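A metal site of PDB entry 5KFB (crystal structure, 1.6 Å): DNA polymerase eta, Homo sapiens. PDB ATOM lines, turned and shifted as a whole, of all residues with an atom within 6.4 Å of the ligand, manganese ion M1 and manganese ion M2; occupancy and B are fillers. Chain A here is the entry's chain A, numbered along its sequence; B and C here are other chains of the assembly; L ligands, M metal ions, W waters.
Residues that only touch manganese ion M1: Ser 116 (3.8 Å). Within 4 Å of manganese ion M1: Asp 16, Ser 116, Asp 118, Glu 119 and DT 8 of chain B. Along chain A the residues within 4 Å of manganese ion M1 span positions 16 to 119.
Manganese ion M2 is bound by OD1 of Asp 16 (2.2 Å), OD2 of Asp 118 (2.2 Å), O of Met 17 (2.2 Å), O1 of the ligand (2.3 Å), O4 of the ligand (2.3 Å) and O7 of the ligand (2.5 Å).
Water W5 lies within hydrogen-bond range of a nitrogen (N2) of the ligand (2.8 Å) and the guanidinium group of Arg 64 (3.5 Å). Water W4 bridges O2 of DT 8 of chain B (2.7 Å) and an oxygen (O11) of the ligand (3.4 Å).
The backbone carbonyl oxygen (O) of Ser 216 is in hydrogen-bond range of the backbone NH (N) of Asp 16. The backbone NH of Glu 119 is in hydrogen-bond range of the side-chain hydroxyl of Ser 116, at 3.2 Å. The side-chain carboxylate (OE1) of Glu 119 is in salt-bridge range of the side-chain amino group (NZ) of Lys 227 (2.8 Å). N of Asp 118 sits at hydrogen-bond distance from OG of Ser 116. The side-chain hydroxyl (OH) of Tyr 55 sits at hydrogen-bond distance from the guanidinium group (NH1) of Arg 58 (3.2 Å). The side-chain amide nitrogen (NE2) of Gln 41 lies within hydrogen-bond range of O2 of DT 4 of chain C (2.8 Å). The guanidinium group of Arg 58 lies within hydrogen-bond range of the backbone carbonyl oxygen of Val 53 (2.9 Å). The guanidinium group of Arg 64 lies within hydrogen-bond range of the backbone carbonyl oxygen of Ile 51.
Asp 18 touches the ligand (CA to O2, 3.5 Å). O of Ile 51 touches C4 of the ligand, at 3.4 Å. Ala 52 touches the ligand (CB to O12, 3.5 Å). Ile 117 touches the ligand (CG2 to O11, 3.8 Å). DA 5 of chain C touches the ligand (N1 to N4, 3.5 Å). Hydrophobic or aromatic side chains within 4 Å of the ligand: Phe 20, Phe 21, Ile 51, Ala 52, Tyr 55 and Ile 117. 17 residues have an atom within 4 Å of the ligand: Asp 16, Met 17, Asp 18, Cys 19, Phe 20, Phe 21, Ile 51, Ala 52, Tyr 55, Arg 58, Arg 64, Ile 117, Asp 118, Lys 234, DT 8 of chain B, DT 4 of chain C and DA 5 of chain C. Along chain A the residues within 4 Å of the ligand span positions 16 to 234. The nearest printed residue that does not touch the ligand is Glu 119 (4.4 Å).
Three residues have an atom within 4 Å of manganese ion M2: Asp 16, Met 17 and Asp 118.
N3 of DT 8 of chain B sits at hydrogen-bond distance from a nitrogen (N3) of the ligand, 3.5 Å away. The side-chain hydroxyl (OH) of Tyr 55 is in hydrogen-bond range of an oxygen (O2) of the ligand. O4 of DT 4 of chain C sits at hydrogen-bond distance from a nitrogen (N3) of the ligand. NZ of Lys 234 lies within salt-bridge range of O3 of the ligand (2.7 Å). N of Cys 19 sits at hydrogen-bond distance from O2 of the ligand (2.8 Å). The guanidinium group of Arg 58 lies within salt-bridge range of an oxygen (O3) of the ligand (3.0 Å). N of Phe 20 lies close to O4 of the ligand (3.0 Å). O5 of the ligand lies within salt-bridge range of NH2 of Arg 64, at 3.1 Å. N of Phe 21 lies within hydrogen-bond range of O12 of the ligand.
Manganese ion M1 is bound by the side-chain carboxylate (OD2) of Asp 16, the side-chain carboxylate (OE2) of Glu 119, water W1, the side-chain carboxylate (OD1) of Asp 118, an oxygen (O7) of the ligand and O3' of DT 8 of chain B. Manganese ion M1 has six donor atoms within binding distance.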
ATOM      1  N   ASP A  16      13.152  10.247  -8.864  1.00  0.00           N
ATOM      2  CA  ASP A  16      12.384  10.880  -7.795  1.00  0.00           C
ATOM      3  C   ASP A  16      11.184  10.028  -7.432  1.00  0.00           C
ATOM      4  O   ASP A  16      10.374   9.673  -8.283  1.00  0.00           O
ATOM      5  CB  ASP A  16      11.911  12.268  -8.213  1.00  0.00           C
ATOM      6  CG  ASP A  16      11.109  12.942  -7.123  1.00  0.00           C
ATOM      7  OD1 ASP A  16       9.886  12.719  -7.086  1.00  0.00           O
ATOM      8  OD2 ASP A  16      11.711  13.672  -6.302  1.00  0.00           O
ATOM      9  N   MET A  17      11.055   9.706  -6.145  1.00  0.00           N
ATOM     10  CA  MET A  17       9.988   8.807  -5.726  1.00  0.00           C
ATOM     11  C   MET A  17       8.605   9.420  -5.890  1.00  0.00           C
ATOM     12  O   MET A  17       8.441  10.603  -5.662  1.00  0.00           O
ATOM     13  CB  MET A  17      10.201   8.366  -4.274  1.00  0.00           C
ATOM     14  CG  MET A  17      11.581   7.806  -4.009  1.00  0.00           C
ATOM     15  SD  MET A  17      12.048   6.413  -5.072  1.00  0.00           S
ATOM     16  CE  MET A  17      10.808   5.238  -4.661  1.00  0.00           C
ATOM     17  N   ASP A  18       7.629   8.617  -6.302  1.00  0.00           N
ATOM     18  CA  ASP A  18       6.260   9.135  -6.411  1.00  0.00           C
ATOM     19  C   ASP A  18       5.605   9.237  -5.044  1.00  0.00           C
ATOM     20  O   ASP A  18       5.636   8.267  -4.271  1.00  0.00           O
ATOM     21  CB  ASP A  18       5.378   8.232  -7.266  1.00  0.00           C
ATOM     22  CG  ASP A  18       5.883   8.095  -8.707  1.00  0.00           C
ATOM     23  OD1 ASP A  18       6.535   9.029  -9.221  1.00  0.00           O
ATOM     24  OD2 ASP A  18       5.587   7.049  -9.305  1.00  0.00           O
ATOM     25  N   CYS A  19       5.037  10.406  -4.764  1.00  0.00           N
ATOM     26  CA  CYS A  19       4.343  10.736  -3.501  1.00  0.00           C
ATOM     27  C   CYS A  19       4.943   9.950  -2.331  1.00  0.00           C
ATOM     28  O   CYS A  19       4.284   9.123  -1.708  1.00  0.00           O
ATOM     29  CB  CYS A  19       2.813  10.489  -3.600  1.00  0.00           C
ATOM     30  SG  CYS A  19       2.222   8.883  -4.170  1.00  0.00           S
ATOM     31  N   PHE A  20       6.222  10.223  -2.069  1.00  0.00           N
ATOM     32  CA  PHE A  20       7.072   9.294  -1.332  1.00  0.00           C
ATOM     33  C   PHE A  20       6.536   8.895   0.050  1.00  0.00           C
ATOM     34  O   PHE A  20       6.388   7.707   0.312  1.00  0.00           O
ATOM     35  CB  PHE A  20       8.493   9.857  -1.181  1.00  0.00           C
ATOM     36  CG  PHE A  20       9.466   8.905  -0.529  1.00  0.00           C
ATOM     37  CD1 PHE A  20       9.525   7.579  -0.915  1.00  0.00           C
ATOM     38  CD2 PHE A  20      10.309   9.337   0.491  1.00  0.00           C
ATOM     39  CE1 PHE A  20      10.438   6.692  -0.315  1.00  0.00           C
ATOM     40  CE2 PHE A  20      11.223   8.457   1.099  1.00  0.00           C
ATOM     41  CZ  PHE A  20      11.280   7.141   0.690  1.00  0.00           C
ATOM     42  N   PHE A  21       6.250   9.867   0.919  1.00  0.00           N
ATOM     43  CA  PHE A  21       5.847   9.482   2.276  1.00  0.00           C
ATOM     44  C   PHE A  21       4.541   8.692   2.234  1.00  0.00           C
ATOM     45  O   PHE A  21       4.319   7.819   3.067  1.00  0.00           O
ATOM     46  CB  PHE A  21       5.671  10.695   3.216  1.00  0.00           C
ATOM     47  CG  PHE A  21       6.943  11.397   3.607  1.00  0.00           C
ATOM     48  CD1 PHE A  21       8.162  11.123   2.979  1.00  0.00           C
ATOM     49  CD2 PHE A  21       6.919  12.318   4.628  1.00  0.00           C
ATOM     50  CE1 PHE A  21       9.323  11.805   3.385  1.00  0.00           C
ATOM     51  CE2 PHE A  21       8.072  12.987   5.048  1.00  0.00           C
ATOM     52  CZ  PHE A  21       9.268  12.731   4.406  1.00  0.00           C
ATOM     53  N   VAL A  22       3.676   8.996   1.274  1.00  0.00           N
ATOM     54  CA  VAL A  22       2.434   8.245   1.124  1.00  0.00           C
ATOM     55  C   VAL A  22       2.743   6.786   0.764  1.00  0.00           C
ATOM     56  O   VAL A  22       2.173   5.859   1.358  1.00  0.00           O
ATOM     57  CB  VAL A  22       1.513   8.882   0.077  1.00  0.00           C
ATOM     58  CG1 VAL A  22       0.425   7.898  -0.392  1.00  0.00           C
ATOM     59  CG2 VAL A  22       0.878  10.171   0.632  1.00  0.00           C
ATOM     60  N   GLN A  41       1.120  15.869   9.584  1.00  0.00           N
ATOM     61  CA  GLN A  41       1.843  15.959  10.851  1.00  0.00           C
ATOM     62  C   GLN A  41       1.068  16.833  11.801  1.00  0.00           C
ATOM     63  O   GLN A  41       0.526  17.880  11.425  1.00  0.00           O
ATOM     64  CB  GLN A  41       3.291  16.437  10.674  1.00  0.00           C
ATOM     65  CG  GLN A  41       3.475  17.711   9.918  1.00  0.00           C
ATOM     66  CD  GLN A  41       4.941  17.943   9.541  1.00  0.00           C
ATOM     67  OE1 GLN A  41       5.807  17.087   9.758  1.00  0.00           O
ATOM     68  NE2 GLN A  41       5.216  19.110   9.005  1.00  0.00           N
ATOM     69  N   ILE A  51       1.671  16.874   4.292  1.00  0.00           N
ATOM     70  CA  ILE A  51       3.001  16.981   3.691  1.00  0.00           C
ATOM     71  C   ILE A  51       3.213  16.060   2.491  1.00  0.00           C
ATOM     72  O   ILE A  51       4.212  16.215   1.786  1.00  0.00           O
ATOM     73  CB  ILE A  51       4.127  16.733   4.709  1.00  0.00           C
ATOM     74  CG1 ILE A  51       4.034  15.338   5.349  1.00  0.00           C
ATOM     75  CG2 ILE A  51       4.129  17.837   5.781  1.00  0.00           C
ATOM     76  CD1 ILE A  51       5.235  15.005   6.247  1.00  0.00           C
ATOM     77  N   ALA A  52       2.295  15.137   2.232  1.00  0.00           N
ATOM     78  CA  ALA A  52       2.375  14.279   1.042  1.00  0.00           C
ATOM     79  C   ALA A  52       0.974  13.807   0.648  1.00  0.00           C
ATOM     80  O   ALA A  52       0.143  13.572   1.526  1.00  0.00           O
ATOM     81  CB  ALA A  52       3.301  13.081   1.274  1.00  0.00           C
ATOM     82  N   VAL A  53       0.722  13.658  -0.654  1.00  0.00           N
ATOM     83  CA  VAL A  53      -0.609  13.408  -1.198  1.00  0.00           C
ATOM     84  C   VAL A  53      -0.572  12.377  -2.311  1.00  0.00           C
ATOM     85  O   VAL A  53       0.191  12.523  -3.279  1.00  0.00           O
ATOM     86  CB  VAL A  53      -1.232  14.707  -1.777  1.00  0.00           C
ATOM     87  CG1 VAL A  53      -2.681  14.480  -2.168  1.00  0.00           C
ATOM     88  CG2 VAL A  53      -1.140  15.853  -0.777  1.00  0.00           C
ATOM     89  N   TYR A  55      -1.814  10.301  -5.654  1.00  0.00           N
ATOM     90  CA  TYR A  55      -2.324  10.842  -6.911  1.00  0.00           C
ATOM     91  C   TYR A  55      -3.844  10.764  -7.000  1.00  0.00           C
ATOM     92  O   TYR A  55      -4.468  11.640  -7.579  1.00  0.00           O
ATOM     93  CB  TYR A  55      -1.651  10.142  -8.098  1.00  0.00           C
ATOM     94  CG  TYR A  55      -0.272  10.732  -8.315  1.00  0.00           C
ATOM     95  CD1 TYR A  55       0.806  10.327  -7.528  1.00  0.00           C
ATOM     96  CD2 TYR A  55      -0.066  11.756  -9.240  1.00  0.00           C
ATOM     97  CE1 TYR A  55       2.053  10.913  -7.660  1.00  0.00           C
ATOM     98  CE2 TYR A  55       1.193  12.332  -9.392  1.00  0.00           C
ATOM     99  CZ  TYR A  55       2.243  11.908  -8.612  1.00  0.00           C
ATOM    100  OH  TYR A  55       3.480  12.491  -8.754  1.00  0.00           O
ATOM    101  N   ARG A  58      -4.918  13.851  -5.206  1.00  0.00           N
ATOM    102  CA  ARG A  58      -4.640  15.083  -5.960  1.00  0.00           C
ATOM    103  C   ARG A  58      -5.763  15.387  -6.948  1.00  0.00           C
ATOM    104  O   ARG A  58      -6.017  16.562  -7.253  1.00  0.00           O
ATOM    105  CB  ARG A  58      -3.319  14.964  -6.709  1.00  0.00           C
ATOM    106  CG  ARG A  58      -2.148  14.822  -5.789  1.00  0.00           C
ATOM    107  CD  ARG A  58      -0.840  14.740  -6.555  1.00  0.00           C
ATOM    108  NE  ARG A  58       0.204  14.238  -5.653  1.00  0.00           N
ATOM    109  CZ  ARG A  58       1.509  14.254  -5.902  1.00  0.00           C
ATOM    110  NH1 ARG A  58       1.983  14.772  -7.023  1.00  0.00           N
ATOM    111  NH2 ARG A  58       2.348  13.750  -4.978  1.00  0.00           N
ATOM    112  N   ARG A  64      -0.146  19.549  -0.770  1.00  0.00           N
ATOM    113  CA  ARG A  64       0.757  19.840   0.316  1.00  0.00           C
ATOM    114  C   ARG A  64       0.429  21.214   0.926  1.00  0.00           C
ATOM    115  O   ARG A  64      -0.070  22.102   0.218  1.00  0.00           O
ATOM    116  CB  ARG A  64       2.202  19.773  -0.183  1.00  0.00           C
ATOM    117  CG  ARG A  64       3.279  20.183   0.794  1.00  0.00           C
ATOM    118  CD  ARG A  64       4.657  19.868   0.213  1.00  0.00           C
ATOM    119  NE  ARG A  64       4.796  18.429   0.080  1.00  0.00           N
ATOM    120  CZ  ARG A  64       5.240  17.781  -0.997  1.00  0.00           C
ATOM    121  NH1 ARG A  64       5.639  18.437  -2.085  1.00  0.00           N
ATOM    122  NH2 ARG A  64       5.289  16.465  -0.977  1.00  0.00           N
ATOM    123  N   LEU A  92      10.873  11.989  11.689  1.00  0.00           N
ATOM    124  CA  LEU A  92      10.830  11.528  10.293  1.00  0.00           C
ATOM    125  C   LEU A  92      11.671  10.271  10.023  1.00  0.00           C
ATOM    126  O   LEU A  92      11.957   9.961   8.877  1.00  0.00           O
ATOM    127  CB  LEU A  92      11.293  12.639   9.359  1.00  0.00           C
ATOM    128  CG  LEU A  92      10.569  13.973   9.550  1.00  0.00           C
ATOM    129  CD1 LEU A  92      11.183  15.054   8.668  1.00  0.00           C
ATOM    130  CD2 LEU A  92       9.101  13.779   9.197  1.00  0.00           C
ATOM    131  N   SER A 116      17.677  14.980  -2.186  1.00  0.00           N
ATOM    132  CA  SER A 116      16.642  15.173  -1.184  1.00  0.00           C
ATOM    133  C   SER A 116      16.345  13.830  -0.529  1.00  0.00           C
ATOM    134  O   SER A 116      16.945  12.813  -0.868  1.00  0.00           O
ATOM    135  CB  SER A 116      15.360  15.723  -1.811  1.00  0.00           C
ATOM    136  OG  SER A 116      14.616  14.668  -2.398  1.00  0.00           O
ATOM    137  N   ILE A 117      15.388  13.805   0.390  1.00  0.00           N
ATOM    138  CA  ILE A 117      15.025  12.563   1.028  1.00  0.00           C
ATOM    139  C   ILE A 117      14.477  11.536   0.010  1.00  0.00           C
ATOM    140  O   ILE A 117      14.506  10.337   0.250  1.00  0.00           O
ATOM    141  CB  ILE A 117      13.991  12.789   2.162  1.00  0.00           C
ATOM    142  CG1 ILE A 117      13.997  11.606   3.140  1.00  0.00           C
ATOM    143  CG2 ILE A 117      12.603  13.071   1.582  1.00  0.00           C
ATOM    144  CD1 ILE A 117      13.205  11.871   4.429  1.00  0.00           C
ATOM    145  N   ASP A 118      13.979  12.009  -1.136  1.00  0.00           N
ATOM    146  CA  ASP A 118      13.373  11.040  -2.052  1.00  0.00           C
ATOM    147  C   ASP A 118      13.902  11.135  -3.487  1.00  0.00           C
ATOM    148  O   ASP A 118      13.257  10.644  -4.421  1.00  0.00           O
ATOM    149  CB  ASP A 118      11.842  11.185  -2.056  1.00  0.00           C
ATOM    150  CG  ASP A 118      11.337  12.214  -3.050  1.00  0.00           C
ATOM    151  OD1 ASP A 118      11.965  13.300  -3.228  1.00  0.00           O
ATOM    152  OD2 ASP A 118      10.314  11.914  -3.714  1.00  0.00           O
ATOM    153  N   GLU A 119      15.064  11.744  -3.685  1.00  0.00           N
ATOM    154  CA  GLU A 119      15.584  11.783  -5.042  1.00  0.00           C
ATOM    155  C   GLU A 119      17.088  11.882  -5.117  1.00  0.00           C
ATOM    156  O   GLU A 119      17.750  12.353  -4.194  1.00  0.00           O
ATOM    157  CB  GLU A 119      14.969  12.947  -5.822  1.00  0.00           C
ATOM    158  CG  GLU A 119      15.547  14.301  -5.510  1.00  0.00           C
ATOM    159  CD  GLU A 119      14.541  15.395  -5.762  1.00  0.00           C
ATOM    160  OE1 GLU A 119      14.641  16.089  -6.787  1.00  0.00           O
ATOM    161  OE2 GLU A 119      13.622  15.553  -4.928  1.00  0.00           O
ATOM    162  N   SER A 216       9.478   8.103 -10.621  1.00  0.00           N
ATOM    163  CA  SER A 216       9.631   8.654 -11.953  1.00  0.00           C
ATOM    164  C   SER A 216      11.073   9.039 -12.168  1.00  0.00           C
ATOM    165  O   SER A 216      11.861   9.067 -11.213  1.00  0.00           O
ATOM    166  CB  SER A 216       8.715   9.859 -12.124  1.00  0.00           C
ATOM    167  OG  SER A 216       7.359   9.452 -11.938  1.00  0.00           O
ATOM    168  N   LYS A 227      16.141  16.866 -14.073  1.00  0.00           N
ATOM    169  CA  LYS A 227      15.117  17.216 -13.090  1.00  0.00           C
ATOM    170  C   LYS A 227      13.830  17.666 -13.762  1.00  0.00           C
ATOM    171  O   LYS A 227      12.728  17.225 -13.410  1.00  0.00           O
ATOM    172  CB  LYS A 227      15.635  18.314 -12.144  1.00  0.00           C
ATOM    173  CG  LYS A 227      14.580  18.778 -11.125  1.00  0.00           C
ATOM    174  CD  LYS A 227      14.083  17.638 -10.229  1.00  0.00           C
ATOM    175  CE  LYS A 227      13.047  18.141  -9.220  1.00  0.00           C
ATOM    176  NZ  LYS A 227      12.551  17.094  -8.272  1.00  0.00           N
ATOM    177  N   LYS A 234       4.529  12.157 -14.666  1.00  0.00           N
ATOM    178  CA  LYS A 234       4.739  11.480 -13.352  1.00  0.00           C
ATOM    179  C   LYS A 234       3.262  11.103 -13.248  1.00  0.00           C
ATOM    180  O   LYS A 234       2.461  11.807 -13.791  1.00  0.00           O
ATOM    181  CB  LYS A 234       5.197  12.288 -12.144  1.00  0.00           C
ATOM    182  CG  LYS A 234       4.754  13.693 -12.124  1.00  0.00           C
ATOM    183  CD  LYS A 234       5.330  14.452 -10.938  1.00  0.00           C
ATOM    184  CE  LYS A 234       4.222  15.279 -10.275  1.00  0.00           C
ATOM    185  NZ  LYS A 234       4.761  16.193  -9.222  1.00  0.00           N
ATOM    186  N   PRO A 235       2.888  10.061 -12.517  1.00  0.00           N
ATOM    187  CA  PRO A 235       3.803   9.184 -11.778  1.00  0.00           C
ATOM    188  C   PRO A 235       4.206   7.948 -12.559  1.00  0.00           C
ATOM    189  O   PRO A 235       3.616   7.666 -13.603  1.00  0.00           O
ATOM    190  CB  PRO A 235       2.975   8.773 -10.571  1.00  0.00           C
ATOM    191  CG  PRO A 235       1.581   8.649 -11.153  1.00  0.00           C
ATOM    192  CD  PRO A 235       1.481   9.732 -12.220  1.00  0.00           C
ATOM    193  P    DT B   8      11.864  21.331  -5.325  1.00  0.00           P
ATOM    194  OP1  DT B   8      11.784  20.514  -6.562  1.00  0.00           O
ATOM    195  OP2  DT B   8      10.678  22.126  -4.893  1.00  0.00           O
ATOM    196  O5'  DT B   8      12.237  20.381  -4.080  1.00  0.00           O
ATOM    197  C5'  DT B   8      13.201  19.293  -4.137  1.00  0.00           C
ATOM    198  C4'  DT B   8      12.935  18.402  -2.935  1.00  0.00           C
ATOM    199  O4'  DT B   8      12.923  19.309  -1.809  1.00  0.00           O
ATOM    200  C3'  DT B   8      11.538  17.804  -3.059  1.00  0.00           C
ATOM    201  O3'  DT B   8      11.593  16.414  -2.826  1.00  0.00           O
ATOM    202  C2'  DT B   8      10.719  18.539  -1.981  1.00  0.00           C
ATOM    203  C1'  DT B   8      11.788  19.029  -1.021  1.00  0.00           C
ATOM    204  N1   DT B   8      11.402  20.265  -0.309  1.00  0.00           N
ATOM    205  C2   DT B   8      11.350  20.248   1.063  1.00  0.00           C
ATOM    206  O2   DT B   8      11.605  19.267   1.717  1.00  0.00           O
ATOM    207  N3   DT B   8      10.971  21.441   1.639  1.00  0.00           N
ATOM    208  C4   DT B   8      10.658  22.617   0.992  1.00  0.00           C
ATOM    209  O4   DT B   8      10.344  23.631   1.598  1.00  0.00           O
ATOM    210  C5   DT B   8      10.721  22.561  -0.450  1.00  0.00           C
ATOM    211  C7   DT B   8      10.415  23.787  -1.263  1.00  0.00           C
ATOM    212  C6   DT B   8      11.093  21.408  -1.021  1.00  0.00           C
ATOM    213  P    DT C   3      -0.433  29.437   8.304  1.00  0.00           P
ATOM    214  OP1  DT C   3       0.252  30.750   8.388  1.00  0.00           O
ATOM    215  OP2  DT C   3      -1.777  29.324   7.720  1.00  0.00           O
ATOM    216  O5'  DT C   3       0.543  28.417   7.557  1.00  0.00           O
ATOM    217  C5'  DT C   3       0.298  27.025   7.620  1.00  0.00           C
ATOM    218  C4'  DT C   3       1.491  26.251   7.102  1.00  0.00           C
ATOM    219  O4'  DT C   3       1.480  26.261   5.664  1.00  0.00           O
ATOM    220  C3'  DT C   3       2.853  26.818   7.538  1.00  0.00           C
ATOM    221  O3'  DT C   3       3.574  25.851   8.294  1.00  0.00           O
ATOM    222  C2'  DT C   3       3.559  27.178   6.213  1.00  0.00           C
ATOM    223  C1'  DT C   3       2.805  26.333   5.201  1.00  0.00           C
ATOM    224  N1   DT C   3       2.778  26.939   3.838  1.00  0.00           N
ATOM    225  C2   DT C   3       3.326  26.235   2.787  1.00  0.00           C
ATOM    226  O2   DT C   3       3.829  25.128   2.913  1.00  0.00           O
ATOM    227  N3   DT C   3       3.249  26.868   1.580  1.00  0.00           N
ATOM    228  C4   DT C   3       2.689  28.107   1.316  1.00  0.00           C
ATOM    229  O4   DT C   3       2.678  28.601   0.198  1.00  0.00           O
ATOM    230  C5   DT C   3       2.140  28.788   2.468  1.00  0.00           C
ATOM    231  C7   DT C   3       1.511  30.142   2.311  1.00  0.00           C
ATOM    232  C6   DT C   3       2.207  28.175   3.659  1.00  0.00           C
ATOM    233  P    DT C   4       3.973  26.175   9.815  1.00  0.00           P
ATOM    234  OP1  DT C   4       2.717  26.406  10.565  1.00  0.00           O
ATOM    235  OP2  DT C   4       5.018  27.223   9.763  1.00  0.00           O
ATOM    236  O5'  DT C   4       4.685  24.847  10.343  1.00  0.00           O
ATOM    237  C5'  DT C   4       3.935  23.762  10.921  1.00  0.00           C
ATOM    238  C4'  DT C   4       4.802  22.500  10.934  1.00  0.00           C
ATOM    239  O4'  DT C   4       5.102  22.167   9.566  1.00  0.00           O
ATOM    240  C3'  DT C   4       6.153  22.675  11.636  1.00  0.00           C
ATOM    241  O3'  DT C   4       6.502  21.458  12.249  1.00  0.00           O
ATOM    242  C2'  DT C   4       7.090  23.025  10.471  1.00  0.00           C
ATOM    243  C1'  DT C   4       6.500  22.150   9.376  1.00  0.00           C
ATOM    244  N1   DT C   4       6.749  22.572   7.988  1.00  0.00           N
ATOM    245  C2   DT C   4       6.941  21.603   7.059  1.00  0.00           C
ATOM    246  O2   DT C   4       7.001  20.426   7.344  1.00  0.00           O
ATOM    247  N3   DT C   4       7.114  22.043   5.783  1.00  0.00           N
ATOM    248  C4   DT C   4       7.075  23.334   5.329  1.00  0.00           C
ATOM    249  O4   DT C   4       7.238  23.617   4.152  1.00  0.00           O
ATOM    250  C5   DT C   4       6.829  24.337   6.353  1.00  0.00           C
ATOM    251  C7   DT C   4       6.774  25.792   5.997  1.00  0.00           C
ATOM    252  C6   DT C   4       6.673  23.907   7.619  1.00  0.00           C
ATOM    253  P    DA C   5       7.868  21.306  13.079  1.00  0.00           P
ATOM    254  OP1  DA C   5       7.551  20.459  14.246  1.00  0.00           O
ATOM    255  OP2  DA C   5       8.488  22.643  13.241  1.00  0.00           O
ATOM    256  O5'  DA C   5       8.816  20.501  12.077  1.00  0.00           O
ATOM    257  C5'  DA C   5       8.515  19.160  11.739  1.00  0.00           C
ATOM    258  C4'  DA C   5       9.619  18.587  10.878  1.00  0.00           C
ATOM    259  O4'  DA C   5       9.576  19.174   9.548  1.00  0.00           O
ATOM    260  C3'  DA C   5      11.034  18.839  11.400  1.00  0.00           C
ATOM    261  O3'  DA C   5      11.819  17.693  11.130  1.00  0.00           O
ATOM    262  C2'  DA C   5      11.493  20.033  10.567  1.00  0.00           C
ATOM    263  C1'  DA C   5      10.846  19.694   9.217  1.00  0.00           C
ATOM    264  N9   DA C   5      10.674  20.837   8.358  1.00  0.00           N
ATOM    265  C8   DA C   5      10.375  22.126   8.720  1.00  0.00           C
ATOM    266  N7   DA C   5      10.267  22.942   7.702  1.00  0.00           N
ATOM    267  C5   DA C   5      10.489  22.130   6.591  1.00  0.00           C
ATOM    268  C6   DA C   5      10.511  22.401   5.212  1.00  0.00           C
ATOM    269  N6   DA C   5      10.289  23.600   4.682  1.00  0.00           N
ATOM    270  N1   DA C   5      10.776  21.372   4.382  1.00  0.00           N
ATOM    271  C2   DA C   5      10.993  20.153   4.902  1.00  0.00           C
ATOM    272  N3   DA C   5      11.001  19.782   6.180  1.00  0.00           N
ATOM    273  C4   DA C   5      10.734  20.844   6.981  1.00  0.00           C
HETATM  274  P1  LIG L   1       5.701  13.686  -6.216  1.00  0.00           P
HETATM  275  O1  LIG L   1       7.206  13.792  -6.285  1.00  0.00           O
HETATM  276  O2  LIG L   1       5.178  12.396  -6.777  1.00  0.00           O
HETATM  277  O3  LIG L   1       5.012  14.881  -6.870  1.00  0.00           O
HETATM  278  P2  LIG L   1       6.229  13.752  -3.409  1.00  0.00           P
HETATM  279  O4  LIG L   1       7.262  12.650  -3.501  1.00  0.00           O
HETATM  280  O5  LIG L   1       5.392  13.622  -2.168  1.00  0.00           O
HETATM  281  O6  LIG L   1       5.246  13.728  -4.683  1.00  0.00           O
HETATM  282  P3  LIG L   1       8.399  15.644  -3.275  1.00  0.00           P
HETATM  283  O7  LIG L   1       9.323  14.910  -4.203  1.00  0.00           O
HETATM  284  O8  LIG L   1       8.368  17.147  -3.516  1.00  0.00           O
HETATM  285  O9  LIG L   1       6.879  15.200  -3.415  1.00  0.00           O
HETATM  286  O10 LIG L   1       8.806  15.421  -1.767  1.00  0.00           O
HETATM  287  C1  LIG L   1       9.192  14.152  -1.298  1.00  0.00           C
HETATM  288  C2  LIG L   1       8.752  13.984   0.152  1.00  0.00           C
HETATM  289  O11 LIG L   1       9.401  14.973   0.926  1.00  0.00           O
HETATM  290  C3  LIG L   1       7.326  14.179   0.334  1.00  0.00           C
HETATM  291  O12 LIG L   1       6.606  12.937   0.191  1.00  0.00           O
HETATM  292  C4  LIG L   1       7.197  14.690   1.702  1.00  0.00           C
HETATM  293  C5  LIG L   1       8.460  15.467   1.893  1.00  0.00           C
HETATM  294  N1  LIG L   1       8.270  16.854   1.664  1.00  0.00           N
HETATM  295  C6  LIG L   1       8.277  17.521   0.484  1.00  0.00           C
HETATM  296  N2  LIG L   1       8.058  18.813   0.663  1.00  0.00           N
HETATM  297  C7  LIG L   1       7.914  19.032   1.982  1.00  0.00           C
HETATM  298  C8  LIG L   1       7.670  20.147   2.774  1.00  0.00           C
HETATM  299  N3  LIG L   1       7.528  21.431   2.148  1.00  0.00           N
HETATM  300  N4  LIG L   1       7.553  20.015   4.093  1.00  0.00           N
HETATM  301  C9  LIG L   1       7.687  18.817   4.710  1.00  0.00           C
HETATM  302  N5  LIG L   1       7.939  17.702   3.971  1.00  0.00           N
HETATM  303  C10 LIG L   1       8.036  17.798   2.633  1.00  0.00           C
HETATM  304 MN    MN M   1      11.562  14.933  -4.685  1.00  0.00          MN
HETATM  305 MN    MN M   2       8.876  12.696  -5.160  1.00  0.00          MN
HETATM  306  O   HOH W   1      10.859  16.493  -6.035  1.00  0.00           O
HETATM  307  O   HOH W   2       4.420  17.133  -5.670  1.00  0.00           O
HETATM  308  O   HOH W   3       2.827  14.531  -2.263  1.00  0.00           O
HETATM  309  O   HOH W   4      11.587  16.817   2.734  1.00  0.00           O
HETATM  310  O   HOH W   5       7.572  21.083  -0.961  1.00  0.00           O
HETATM  311  O   HOH W   6       9.125  16.010   5.872  1.00  0.00           O
HETATM  312  O   HOH W   7       8.449  15.858  -7.417  1.00  0.00           O
HETATM  313  O   HOH W   8      11.873  15.789  -0.387  1.00  0.00           O
